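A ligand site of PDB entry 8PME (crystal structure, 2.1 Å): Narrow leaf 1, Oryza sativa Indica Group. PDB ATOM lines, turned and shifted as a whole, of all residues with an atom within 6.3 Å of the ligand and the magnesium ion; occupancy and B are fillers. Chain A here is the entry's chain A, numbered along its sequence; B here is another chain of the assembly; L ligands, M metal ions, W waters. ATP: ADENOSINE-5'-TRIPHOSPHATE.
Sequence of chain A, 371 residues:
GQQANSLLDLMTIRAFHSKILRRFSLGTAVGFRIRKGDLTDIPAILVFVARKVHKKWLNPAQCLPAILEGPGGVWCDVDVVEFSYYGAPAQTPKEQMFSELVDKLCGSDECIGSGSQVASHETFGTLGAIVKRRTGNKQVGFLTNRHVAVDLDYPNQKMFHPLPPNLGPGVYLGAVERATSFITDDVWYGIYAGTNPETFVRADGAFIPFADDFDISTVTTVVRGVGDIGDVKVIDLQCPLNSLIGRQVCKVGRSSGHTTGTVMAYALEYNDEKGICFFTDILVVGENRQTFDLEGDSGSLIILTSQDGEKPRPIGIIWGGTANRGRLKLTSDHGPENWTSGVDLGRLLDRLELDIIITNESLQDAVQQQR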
ATOM      1  N   PHE A  24      12.061 -22.276 -33.103  1.00  0.00           N
ATOM      2  CA  PHE A  24      11.679 -21.573 -31.872  1.00  0.00           C
ATOM      3  C   PHE A  24      12.198 -22.269 -30.618  1.00  0.00           C
ATOM      4  O   PHE A  24      11.588 -22.163 -29.560  1.00  0.00           O
ATOM      5  CB  PHE A  24      10.171 -21.408 -31.791  1.00  0.00           C
ATOM      6  CG  PHE A  24       9.578 -20.650 -32.945  1.00  0.00           C
ATOM      7  CD1 PHE A  24       9.749 -19.288 -33.062  1.00  0.00           C
ATOM      8  CD2 PHE A  24       8.832 -21.306 -33.915  1.00  0.00           C
ATOM      9  CE1 PHE A  24       9.199 -18.587 -34.117  1.00  0.00           C
ATOM     10  CE2 PHE A  24       8.287 -20.613 -34.975  1.00  0.00           C
ATOM     11  CZ  PHE A  24       8.467 -19.256 -35.075  1.00  0.00           C
ATOM     12  N   SER A  25      13.320 -22.975 -30.717  1.00  0.00           N
ATOM     13  CA  SER A  25      13.818 -23.729 -29.570  1.00  0.00           C
ATOM     14  C   SER A  25      15.308 -23.476 -29.374  1.00  0.00           C
ATOM     15  O   SER A  25      16.021 -23.106 -30.308  1.00  0.00           O
ATOM     16  CB  SER A  25      13.588 -25.235 -29.764  1.00  0.00           C
ATOM     17  OG  SER A  25      14.395 -25.756 -30.798  1.00  0.00           O
ATOM     18  N   ARG A  33       9.183 -38.945 -22.953  1.00  0.00           N
ATOM     19  CA  ARG A  33       8.419 -37.764 -22.592  1.00  0.00           C
ATOM     20  C   ARG A  33       8.424 -37.573 -21.082  1.00  0.00           C
ATOM     21  O   ARG A  33       8.254 -38.521 -20.316  1.00  0.00           O
ATOM     22  CB  ARG A  33       6.971 -37.857 -23.098  1.00  0.00           C
ATOM     23  CG  ARG A  33       6.098 -36.709 -22.607  1.00  0.00           C
ATOM     24  CD  ARG A  33       4.622 -36.904 -22.932  1.00  0.00           C
ATOM     25  NE  ARG A  33       4.329 -36.743 -24.356  1.00  0.00           N
ATOM     26  CZ  ARG A  33       4.233 -35.567 -24.974  1.00  0.00           C
ATOM     27  NH1 ARG A  33       4.419 -34.444 -24.290  1.00  0.00           N
ATOM     28  NH2 ARG A  33       3.959 -35.523 -26.273  1.00  0.00           N
ATOM     29  N   ILE A  34       8.610 -36.320 -20.661  1.00  0.00           N
ATOM     30  CA  ILE A  34       8.565 -35.947 -19.258  1.00  0.00           C
ATOM     31  C   ILE A  34       7.250 -35.227 -19.012  1.00  0.00           C
ATOM     32  O   ILE A  34       6.954 -34.222 -19.669  1.00  0.00           O
ATOM     33  CB  ILE A  34       9.757 -35.058 -18.863  1.00  0.00           C
ATOM     34  CG1 ILE A  34      11.072 -35.682 -19.325  1.00  0.00           C
ATOM     35  CG2 ILE A  34       9.776 -34.817 -17.353  1.00  0.00           C
ATOM     36  CD1 ILE A  34      12.286 -34.809 -19.044  1.00  0.00           C
ATOM     37  N   ARG A  35       6.451 -35.734 -18.071  1.00  0.00           N
ATOM     38  CA  ARG A  35       5.135 -35.181 -17.781  1.00  0.00           C
ATOM     39  C   ARG A  35       4.958 -35.023 -16.279  1.00  0.00           C
ATOM     40  O   ARG A  35       5.197 -35.970 -15.520  1.00  0.00           O
ATOM     41  CB  ARG A  35       4.036 -36.086 -18.364  1.00  0.00           C
ATOM     42  CG  ARG A  35       2.633 -35.675 -17.983  1.00  0.00           C
ATOM     43  CD  ARG A  35       1.641 -36.505 -18.777  1.00  0.00           C
ATOM     44  NE  ARG A  35       1.670 -36.174 -20.192  1.00  0.00           N
ATOM     45  CZ  ARG A  35       1.393 -37.023 -21.167  1.00  0.00           C
ATOM     46  NH1 ARG A  35       1.078 -38.277 -20.882  1.00  0.00           N
ATOM     47  NH2 ARG A  35       1.435 -36.626 -22.432  1.00  0.00           N
ATOM     48  N   LYS A  36       4.554 -33.826 -15.869  1.00  0.00           N
ATOM     49  CA  LYS A  36       4.353 -33.514 -14.452  1.00  0.00           C
ATOM     50  C   LYS A  36       5.594 -33.855 -13.638  1.00  0.00           C
ATOM     51  O   LYS A  36       5.521 -34.359 -12.516  1.00  0.00           O
ATOM     52  CB  LYS A  36       3.120 -34.238 -13.898  1.00  0.00           C
ATOM     53  CG  LYS A  36       1.832 -33.874 -14.630  1.00  0.00           C
ATOM     54  CD  LYS A  36       0.721 -34.867 -14.304  1.00  0.00           C
ATOM     55  CE  LYS A  36      -0.551 -34.516 -15.062  1.00  0.00           C
ATOM     56  NZ  LYS A  36      -1.041 -33.151 -14.733  1.00  0.00           N
ATOM     57  N   GLY A  37       6.762 -33.574 -14.216  1.00  0.00           N
ATOM     58  CA  GLY A  37       8.030 -33.761 -13.539  1.00  0.00           C
ATOM     59  C   GLY A  37       8.547 -35.180 -13.518  1.00  0.00           C
ATOM     60  O   GLY A  37       9.668 -35.410 -13.041  1.00  0.00           O
ATOM     61  N   VAL A  49      13.155 -25.069 -24.542  1.00  0.00           N
ATOM     62  CA  VAL A  49      12.806 -23.675 -24.735  1.00  0.00           C
ATOM     63  C   VAL A  49      13.237 -22.878 -23.516  1.00  0.00           C
ATOM     64  O   VAL A  49      13.287 -23.392 -22.393  1.00  0.00           O
ATOM     65  CB  VAL A  49      11.294 -23.502 -24.997  1.00  0.00           C
ATOM     66  CG1 VAL A  49      10.872 -24.309 -26.213  1.00  0.00           C
ATOM     67  CG2 VAL A  49      10.504 -23.923 -23.765  1.00  0.00           C
ATOM     68  N   ARG A  51      11.667 -20.476 -21.976  1.00  0.00           N
ATOM     69  CA  ARG A  51      10.541 -20.363 -21.054  1.00  0.00           C
ATOM     70  C   ARG A  51       9.354 -21.103 -21.636  1.00  0.00           C
ATOM     71  O   ARG A  51       8.936 -20.816 -22.764  1.00  0.00           O
ATOM     72  CB  ARG A  51      10.198 -18.888 -20.776  1.00  0.00           C
ATOM     73  CG  ARG A  51       8.909 -18.661 -19.999  1.00  0.00           C
ATOM     74  CD  ARG A  51       8.913 -19.399 -18.672  1.00  0.00           C
ATOM     75  NE  ARG A  51       7.603 -19.374 -18.032  1.00  0.00           N
ATOM     76  CZ  ARG A  51       7.220 -20.217 -17.074  1.00  0.00           C
ATOM     77  NH1 ARG A  51       8.054 -21.161 -16.650  1.00  0.00           N
ATOM     78  NH2 ARG A  51       6.001 -20.133 -16.557  1.00  0.00           N
ATOM     79  N   LYS A  52       8.798 -22.036 -20.870  1.00  0.00           N
ATOM     80  CA  LYS A  52       7.626 -22.794 -21.298  1.00  0.00           C
ATOM     81  C   LYS A  52       6.375 -22.064 -20.819  1.00  0.00           C
ATOM     82  O   LYS A  52       6.220 -21.816 -19.620  1.00  0.00           O
ATOM     83  CB  LYS A  52       7.702 -24.210 -20.724  1.00  0.00           C
ATOM     84  CG  LYS A  52       6.570 -25.156 -21.101  1.00  0.00           C
ATOM     85  CD  LYS A  52       6.944 -26.574 -20.679  1.00  0.00           C
ATOM     86  CE  LYS A  52       5.782 -27.536 -20.769  1.00  0.00           C
ATOM     87  NZ  LYS A  52       6.187 -28.901 -20.319  1.00  0.00           N
ATOM     88  N   VAL A  53       5.483 -21.731 -21.755  1.00  0.00           N
ATOM     89  CA  VAL A  53       4.312 -20.915 -21.467  1.00  0.00           C
ATOM     90  C   VAL A  53       3.065 -21.598 -22.006  1.00  0.00           C
ATOM     91  O   VAL A  53       3.122 -22.488 -22.855  1.00  0.00           O
ATOM     92  CB  VAL A  53       4.431 -19.484 -22.034  1.00  0.00           C
ATOM     93  CG1 VAL A  53       5.734 -18.838 -21.587  1.00  0.00           C
ATOM     94  CG2 VAL A  53       4.325 -19.497 -23.554  1.00  0.00           C
ATOM     95  N   HIS A  54       1.922 -21.149 -21.500  1.00  0.00           N
ATOM     96  CA  HIS A  54       0.632 -21.691 -21.890  1.00  0.00           C
ATOM     97  C   HIS A  54       0.355 -21.417 -23.364  1.00  0.00           C
ATOM     98  O   HIS A  54       0.816 -20.432 -23.938  1.00  0.00           O
ATOM     99  CB  HIS A  54      -0.467 -21.094 -21.016  1.00  0.00           C
ATOM    100  CG  HIS A  54      -1.799 -21.764 -21.144  1.00  0.00           C
ATOM    101  ND1 HIS A  54      -2.665 -21.517 -22.186  1.00  0.00           N
ATOM    102  CD2 HIS A  54      -2.429 -22.655 -20.345  1.00  0.00           C
ATOM    103  CE1 HIS A  54      -3.760 -22.233 -22.028  1.00  0.00           C
ATOM    104  NE2 HIS A  54      -3.642 -22.941 -20.920  1.00  0.00           N
ATOM    105  N   LYS A  55      -0.423 -22.320 -23.990  1.00  0.00           N
ATOM    106  CA  LYS A  55      -0.722 -22.181 -25.407  1.00  0.00           C
ATOM    107  C   LYS A  55      -1.336 -20.826 -25.747  1.00  0.00           C
ATOM    108  O   LYS A  55      -1.143 -20.324 -26.862  1.00  0.00           O
ATOM    109  CB  LYS A  55      -1.691 -23.295 -25.853  1.00  0.00           C
ATOM    110  CG  LYS A  55      -1.062 -24.624 -26.232  1.00  0.00           C
ATOM    111  CD  LYS A  55      -2.142 -25.558 -26.777  1.00  0.00           C
ATOM    112  CE  LYS A  55      -1.565 -26.857 -27.321  1.00  0.00           C
ATOM    113  NZ  LYS A  55      -2.621 -27.702 -27.953  1.00  0.00           N
ATOM    114  N   LYS A  56      -2.080 -20.236 -24.817  1.00  0.00           N
ATOM    115  CA  LYS A  56      -2.788 -18.994 -25.113  1.00  0.00           C
ATOM    116  C   LYS A  56      -1.843 -17.839 -25.443  1.00  0.00           C
ATOM    117  O   LYS A  56      -2.271 -16.877 -26.092  1.00  0.00           O
ATOM    118  CB  LYS A  56      -3.685 -18.594 -23.943  1.00  0.00           C
ATOM    119  CG  LYS A  56      -5.124 -19.104 -24.060  1.00  0.00           C
ATOM    120  CD  LYS A  56      -6.043 -18.428 -23.050  1.00  0.00           C
ATOM    121  CE  LYS A  56      -7.491 -18.878 -23.222  1.00  0.00           C
ATOM    122  NZ  LYS A  56      -7.698 -20.287 -22.779  1.00  0.00           N
ATOM    123  N   LEU A  58       1.083 -18.288 -27.137  1.00  0.00           N
ATOM    124  CA  LEU A  58       1.903 -18.677 -28.272  1.00  0.00           C
ATOM    125  C   LEU A  58       1.185 -18.391 -29.573  1.00  0.00           C
ATOM    126  O   LEU A  58      -0.034 -18.599 -29.684  1.00  0.00           O
ATOM    127  CB  LEU A  58       2.258 -20.166 -28.190  1.00  0.00           C
ATOM    128  CG  LEU A  58       3.179 -20.581 -27.037  1.00  0.00           C
ATOM    129  CD1 LEU A  58       3.217 -22.097 -26.912  1.00  0.00           C
ATOM    130  CD2 LEU A  58       4.575 -20.025 -27.252  1.00  0.00           C
ATOM    131  N   GLN A  62       4.499 -20.813 -33.525  1.00  0.00           N
ATOM    132  CA  GLN A  62       5.484 -21.234 -32.541  1.00  0.00           C
ATOM    133  C   GLN A  62       5.023 -22.384 -31.657  1.00  0.00           C
ATOM    134  O   GLN A  62       5.857 -22.972 -30.966  1.00  0.00           O
ATOM    135  CB  GLN A  62       5.902 -20.046 -31.658  1.00  0.00           C
ATOM    136  CG  GLN A  62       4.766 -19.243 -31.070  1.00  0.00           C
ATOM    137  CD  GLN A  62       5.241 -17.925 -30.481  1.00  0.00           C
ATOM    138  OE1 GLN A  62       4.437 -17.063 -30.124  1.00  0.00           O
ATOM    139  NE2 GLN A  62       6.561 -17.765 -30.372  1.00  0.00           N
ATOM    140  N   CYS A  63       3.734 -22.734 -31.662  1.00  0.00           N
ATOM    141  CA  CYS A  63       3.256 -23.795 -30.783  1.00  0.00           C
ATOM    142  C   CYS A  63       3.696 -25.139 -31.341  1.00  0.00           C
ATOM    143  O   CYS A  63       3.348 -25.497 -32.476  1.00  0.00           O
ATOM    144  CB  CYS A  63       1.740 -23.745 -30.621  1.00  0.00           C
ATOM    145  SG  CYS A  63       1.128 -24.947 -29.423  1.00  0.00           S
ATOM    146  N   LEU A  64       4.464 -25.877 -30.551  1.00  0.00           N
ATOM    147  CA  LEU A  64       4.963 -27.169 -30.977  1.00  0.00           C
ATOM    148  C   LEU A  64       3.825 -28.184 -31.029  1.00  0.00           C
ATOM    149  O   LEU A  64       2.913 -28.143 -30.192  1.00  0.00           O
ATOM    150  CB  LEU A  64       6.065 -27.655 -30.034  1.00  0.00           C
ATOM    151  CG  LEU A  64       7.373 -26.890 -30.217  1.00  0.00           C
ATOM    152  CD1 LEU A  64       8.207 -26.956 -28.957  1.00  0.00           C
ATOM    153  CD2 LEU A  64       8.149 -27.451 -31.394  1.00  0.00           C
ATOM    154  N   PRO A  65       3.853 -29.118 -31.975  1.00  0.00           N
ATOM    155  CA  PRO A  65       2.863 -30.196 -31.987  1.00  0.00           C
ATOM    156  C   PRO A  65       3.192 -31.244 -30.931  1.00  0.00           C
ATOM    157  O   PRO A  65       4.305 -31.316 -30.414  1.00  0.00           O
ATOM    158  CB  PRO A  65       2.999 -30.786 -33.390  1.00  0.00           C
ATOM    159  CG  PRO A  65       4.458 -30.581 -33.712  1.00  0.00           C
ATOM    160  CD  PRO A  65       4.850 -29.282 -33.049  1.00  0.00           C
ATOM    161  N   ALA A  66       2.193 -32.052 -30.620  1.00  0.00           N
ATOM    162  CA  ALA A  66       2.376 -33.096 -29.616  1.00  0.00           C
ATOM    163  C   ALA A  66       2.938 -34.378 -30.216  1.00  0.00           C
ATOM    164  O   ALA A  66       3.560 -35.162 -29.484  1.00  0.00           O
ATOM    165  CB  ALA A  66       1.058 -33.391 -28.912  1.00  0.00           C
ATOM    166  N   VAL A  78       6.303 -35.329 -28.967  1.00  0.00           N
ATOM    167  CA  VAL A  78       7.148 -34.147 -28.800  1.00  0.00           C
ATOM    168  C   VAL A  78       6.871 -33.593 -27.406  1.00  0.00           C
ATOM    169  O   VAL A  78       5.714 -33.344 -27.053  1.00  0.00           O
ATOM    170  CB  VAL A  78       6.884 -33.088 -29.875  1.00  0.00           C
ATOM    171  CG1 VAL A  78       7.688 -31.828 -29.584  1.00  0.00           C
ATOM    172  CG2 VAL A  78       7.232 -33.643 -31.248  1.00  0.00           C
ATOM    173  N   ASP A  79       7.932 -33.397 -26.638  1.00  0.00           N
ATOM    174  CA  ASP A  79       7.838 -32.980 -25.241  1.00  0.00           C
ATOM    175  C   ASP A  79       8.625 -31.699 -25.052  1.00  0.00           C
ATOM    176  O   ASP A  79       9.766 -31.596 -25.515  1.00  0.00           O
ATOM    177  CB  ASP A  79       8.357 -34.061 -24.289  1.00  0.00           C
ATOM    178  CG  ASP A  79       7.884 -33.845 -22.868  1.00  0.00           C
ATOM    179  OD1 ASP A  79       6.657 -33.737 -22.661  1.00  0.00           O
ATOM    180  OD2 ASP A  79       8.712 -33.778 -21.937  1.00  0.00           O
ATOM    181  N   VAL A  80       8.030 -30.718 -24.379  1.00  0.00           N
ATOM    182  CA  VAL A  80       8.639 -29.410 -24.203  1.00  0.00           C
ATOM    183  C   VAL A  80       9.244 -29.336 -22.813  1.00  0.00           C
ATOM    184  O   VAL A  80       8.573 -29.621 -21.810  1.00  0.00           O
ATOM    185  CB  VAL A  80       7.598 -28.291 -24.412  1.00  0.00           C
ATOM    186  CG1 VAL A  80       8.268 -26.923 -24.367  1.00  0.00           C
ATOM    187  CG2 VAL A  80       6.844 -28.513 -25.717  1.00  0.00           C
ATOM    188  N   VAL A  81      10.512 -28.936 -22.741  1.00  0.00           N
ATOM    189  CA  VAL A  81      11.264 -28.850 -21.497  1.00  0.00           C
ATOM    190  C   VAL A  81      11.862 -27.460 -21.369  1.00  0.00           C
ATOM    191  O   VAL A  81      12.533 -26.978 -22.285  1.00  0.00           O
ATOM    192  CB  VAL A  81      12.356 -29.927 -21.421  1.00  0.00           C
ATOM    193  CG1 VAL A  81      13.184 -29.752 -20.162  1.00  0.00           C
ATOM    194  CG2 VAL A  81      11.739 -31.312 -21.454  1.00  0.00           C
ATOM    195  N   PRO B 169       8.339 -15.893 -25.818  1.00  0.00           N
ATOM    196  CA  PRO B 169       6.951 -15.708 -26.264  1.00  0.00           C
ATOM    197  C   PRO B 169       6.146 -14.885 -25.272  1.00  0.00           C
ATOM    198  O   PRO B 169       6.468 -14.763 -24.092  1.00  0.00           O
ATOM    199  CB  PRO B 169       6.422 -17.141 -26.350  1.00  0.00           C
ATOM    200  CG  PRO B 169       7.214 -17.878 -25.309  1.00  0.00           C
ATOM    201  CD  PRO B 169       8.585 -17.253 -25.316  1.00  0.00           C
HETATM  202  PG  ATP L   1       4.028 -31.493 -18.827  1.00  0.00           P
HETATM  203  O1G ATP L   1       3.838 -30.053 -19.222  1.00  0.00           O
HETATM  204  O2G ATP L   1       5.341 -32.100 -19.294  1.00  0.00           O
HETATM  205  O3G ATP L   1       3.665 -31.838 -17.403  1.00  0.00           O
HETATM  206  PB  ATP L   1       3.332 -32.847 -21.158  1.00  0.00           P
HETATM  207  O1B ATP L   1       2.211 -33.748 -21.609  1.00  0.00           O
HETATM  208  O2B ATP L   1       4.751 -33.368 -21.097  1.00  0.00           O
HETATM  209  O3B ATP L   1       2.928 -32.275 -19.701  1.00  0.00           O
HETATM  210  PA  ATP L   1       4.658 -30.999 -22.754  1.00  0.00           P
HETATM  211  O1A ATP L   1       4.781 -31.568 -24.141  1.00  0.00           O
HETATM  212  O2A ATP L   1       5.806 -31.131 -21.773  1.00  0.00           O
HETATM  213  O3A ATP L   1       3.303 -31.512 -22.041  1.00  0.00           O
HETATM  214  O5' ATP L   1       4.341 -29.434 -22.912  1.00  0.00           O
HETATM  215  C5' ATP L   1       3.530 -28.948 -23.978  1.00  0.00           C
HETATM  216  C4' ATP L   1       3.249 -27.509 -23.616  1.00  0.00           C
HETATM  217  O4' ATP L   1       4.374 -26.711 -23.962  1.00  0.00           O
HETATM  218  C3' ATP L   1       2.050 -26.900 -24.315  1.00  0.00           C
HETATM  219  O3' ATP L   1       0.913 -26.998 -23.467  1.00  0.00           O
HETATM  220  C2' ATP L   1       2.442 -25.452 -24.520  1.00  0.00           C
HETATM  221  O2' ATP L   1       1.811 -24.664 -23.505  1.00  0.00           O
HETATM  222  C1' ATP L   1       3.943 -25.393 -24.308  1.00  0.00           C
HETATM  223  N9  ATP L   1       4.622 -24.968 -25.562  1.00  0.00           N
HETATM  224  C8  ATP L   1       4.345 -25.402 -26.800  1.00  0.00           C
HETATM  225  N7  ATP L   1       5.144 -24.803 -27.718  1.00  0.00           N
HETATM  226  C5  ATP L   1       5.964 -23.963 -27.066  1.00  0.00           C
HETATM  227  C6  ATP L   1       7.048 -23.031 -27.424  1.00  0.00           C
HETATM  228  N6  ATP L   1       7.430 -22.866 -28.711  1.00  0.00           N
HETATM  229  N1  ATP L   1       7.641 -22.335 -26.427  1.00  0.00           N
HETATM  230  C2  ATP L   1       7.262 -22.487 -25.137  1.00  0.00           C
HETATM  231  N3  ATP L   1       6.288 -23.314 -24.739  1.00  0.00           N
HETATM  232  C4  ATP L   1       5.611 -24.071 -25.641  1.00  0.00           C
HETATM  233 MG    MG M   1       6.749 -32.906 -20.848  1.00  0.00          MG
HETATM  234  O   HOH W   1       8.368 -31.655 -20.669  1.00  0.00           O
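The backbone NH of Val 53 lies within hydrogen-bond range of a nitrogen (N3) of the ligand (3.5 Å).
An oxygen (O2') of the ligand lies within hydrogen-bond range of the backbone carbonyl oxygen of Val 53 (2.6 Å).
N of Lys 36 is in hydrogen-bond range of O3G of the ligand (2.7 Å).
O1G of the ligand is in salt-bridge range of NZ of Lys 52 (2.8 Å).
The backbone carbonyl oxygen (O) of Gln 62 sits at hydrogen-bond distance from a nitrogen (N6) of the ligand (2.8 Å).
The guanidinium group of Arg 35 is in salt-bridge range of an oxygen (O1B) of the ligand (2.9 Å).
O1A of the ligand is in salt-bridge range of NH1 of Arg 33 (2.9 Å).
N7 of the ligand lies within hydrogen-bond range of N of Leu 64, at 3.1 Å.
O1A of the ligand sits at hydrogen-bond distance from N of Val 80 (3.4 Å).
The backbone NH (N) of Lys 55 is in hydrogen-bond range of an oxygen (O2') of the ligand (3.3 Å).
The side-chain carboxylate (OD1) of Asp 79 lies close to the guanidinium group (NH1) of Arg 33, at 2.9 Å.
The side-chain amino group of Lys 52 is in hydrogen-bond range of the backbone carbonyl oxygen of Val 80 (2.9 Å).
The guanidinium group (NH2) of Arg 33 sits at hydrogen-bond distance from the backbone carbonyl oxygen (O) of Val 78, 2.9 Å away.
The backbone carbonyl oxygen (O) of Ala 66 sits at hydrogen-bond distance from the guanidinium group (NH2) of Arg 33, at 3.3 Å.
N of Val 78 sits at hydrogen-bond distance from O of Ala 66 (2.8 Å).
A ring nitrogen (ND1) of His 54 sits at hydrogen-bond distance from the backbone NH of Lys 56 (3.0 Å).
The backbone NH of Val 49 sits at hydrogen-bond distance from the backbone carbonyl oxygen of Val 81 (3.0 Å).
Val 49 touches the ligand.
O of Arg 51 touches C2 of the ligand, 3.4 Å away.
His 54 touches the ligand.
Leu 58 touches the ligand (CD1 to C5, 3.3 Å).
CA of Cys 63 touches N7 of the ligand (3.7 Å).
O of Val 78 touches O1A of the ligand, 3.5 Å away.
17 residues have an atom within 4 Å of the ligand: Arg 33, Ile 34, Arg 35, Lys 36, Val 49, Arg 51, Lys 52, Val 53, His 54, Lys 55, Leu 58, Gln 62, Cys 63, Leu 64, Val 78, Asp 79 and Val 80.
Along chain A the residues within 4 Å of the ligand span positions 33 to 80.
Merely in contact with the magnesium ion: Val 80 and Arg 35.
Four residues have an atom within 4 Å of the magnesium ion: Ile 34, Arg 35, Asp 79 and Val 80.
The nearest printed residue that does not touch the magnesium ion is Lys 52 (4.1 Å).
The magnesium ion is bound by O of Ile 34 (1.8 Å), OD1 of Asp 79 (2.0 Å), water W1 (2.1 Å), O2B of the ligand (2.1 Å), O2A of the ligand (2.2 Å), O2G of the ligand (2.2 Å) and OD2 of Asp 79 (2.4 Å).
The magnesium ion has seven donor atoms within binding distance.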
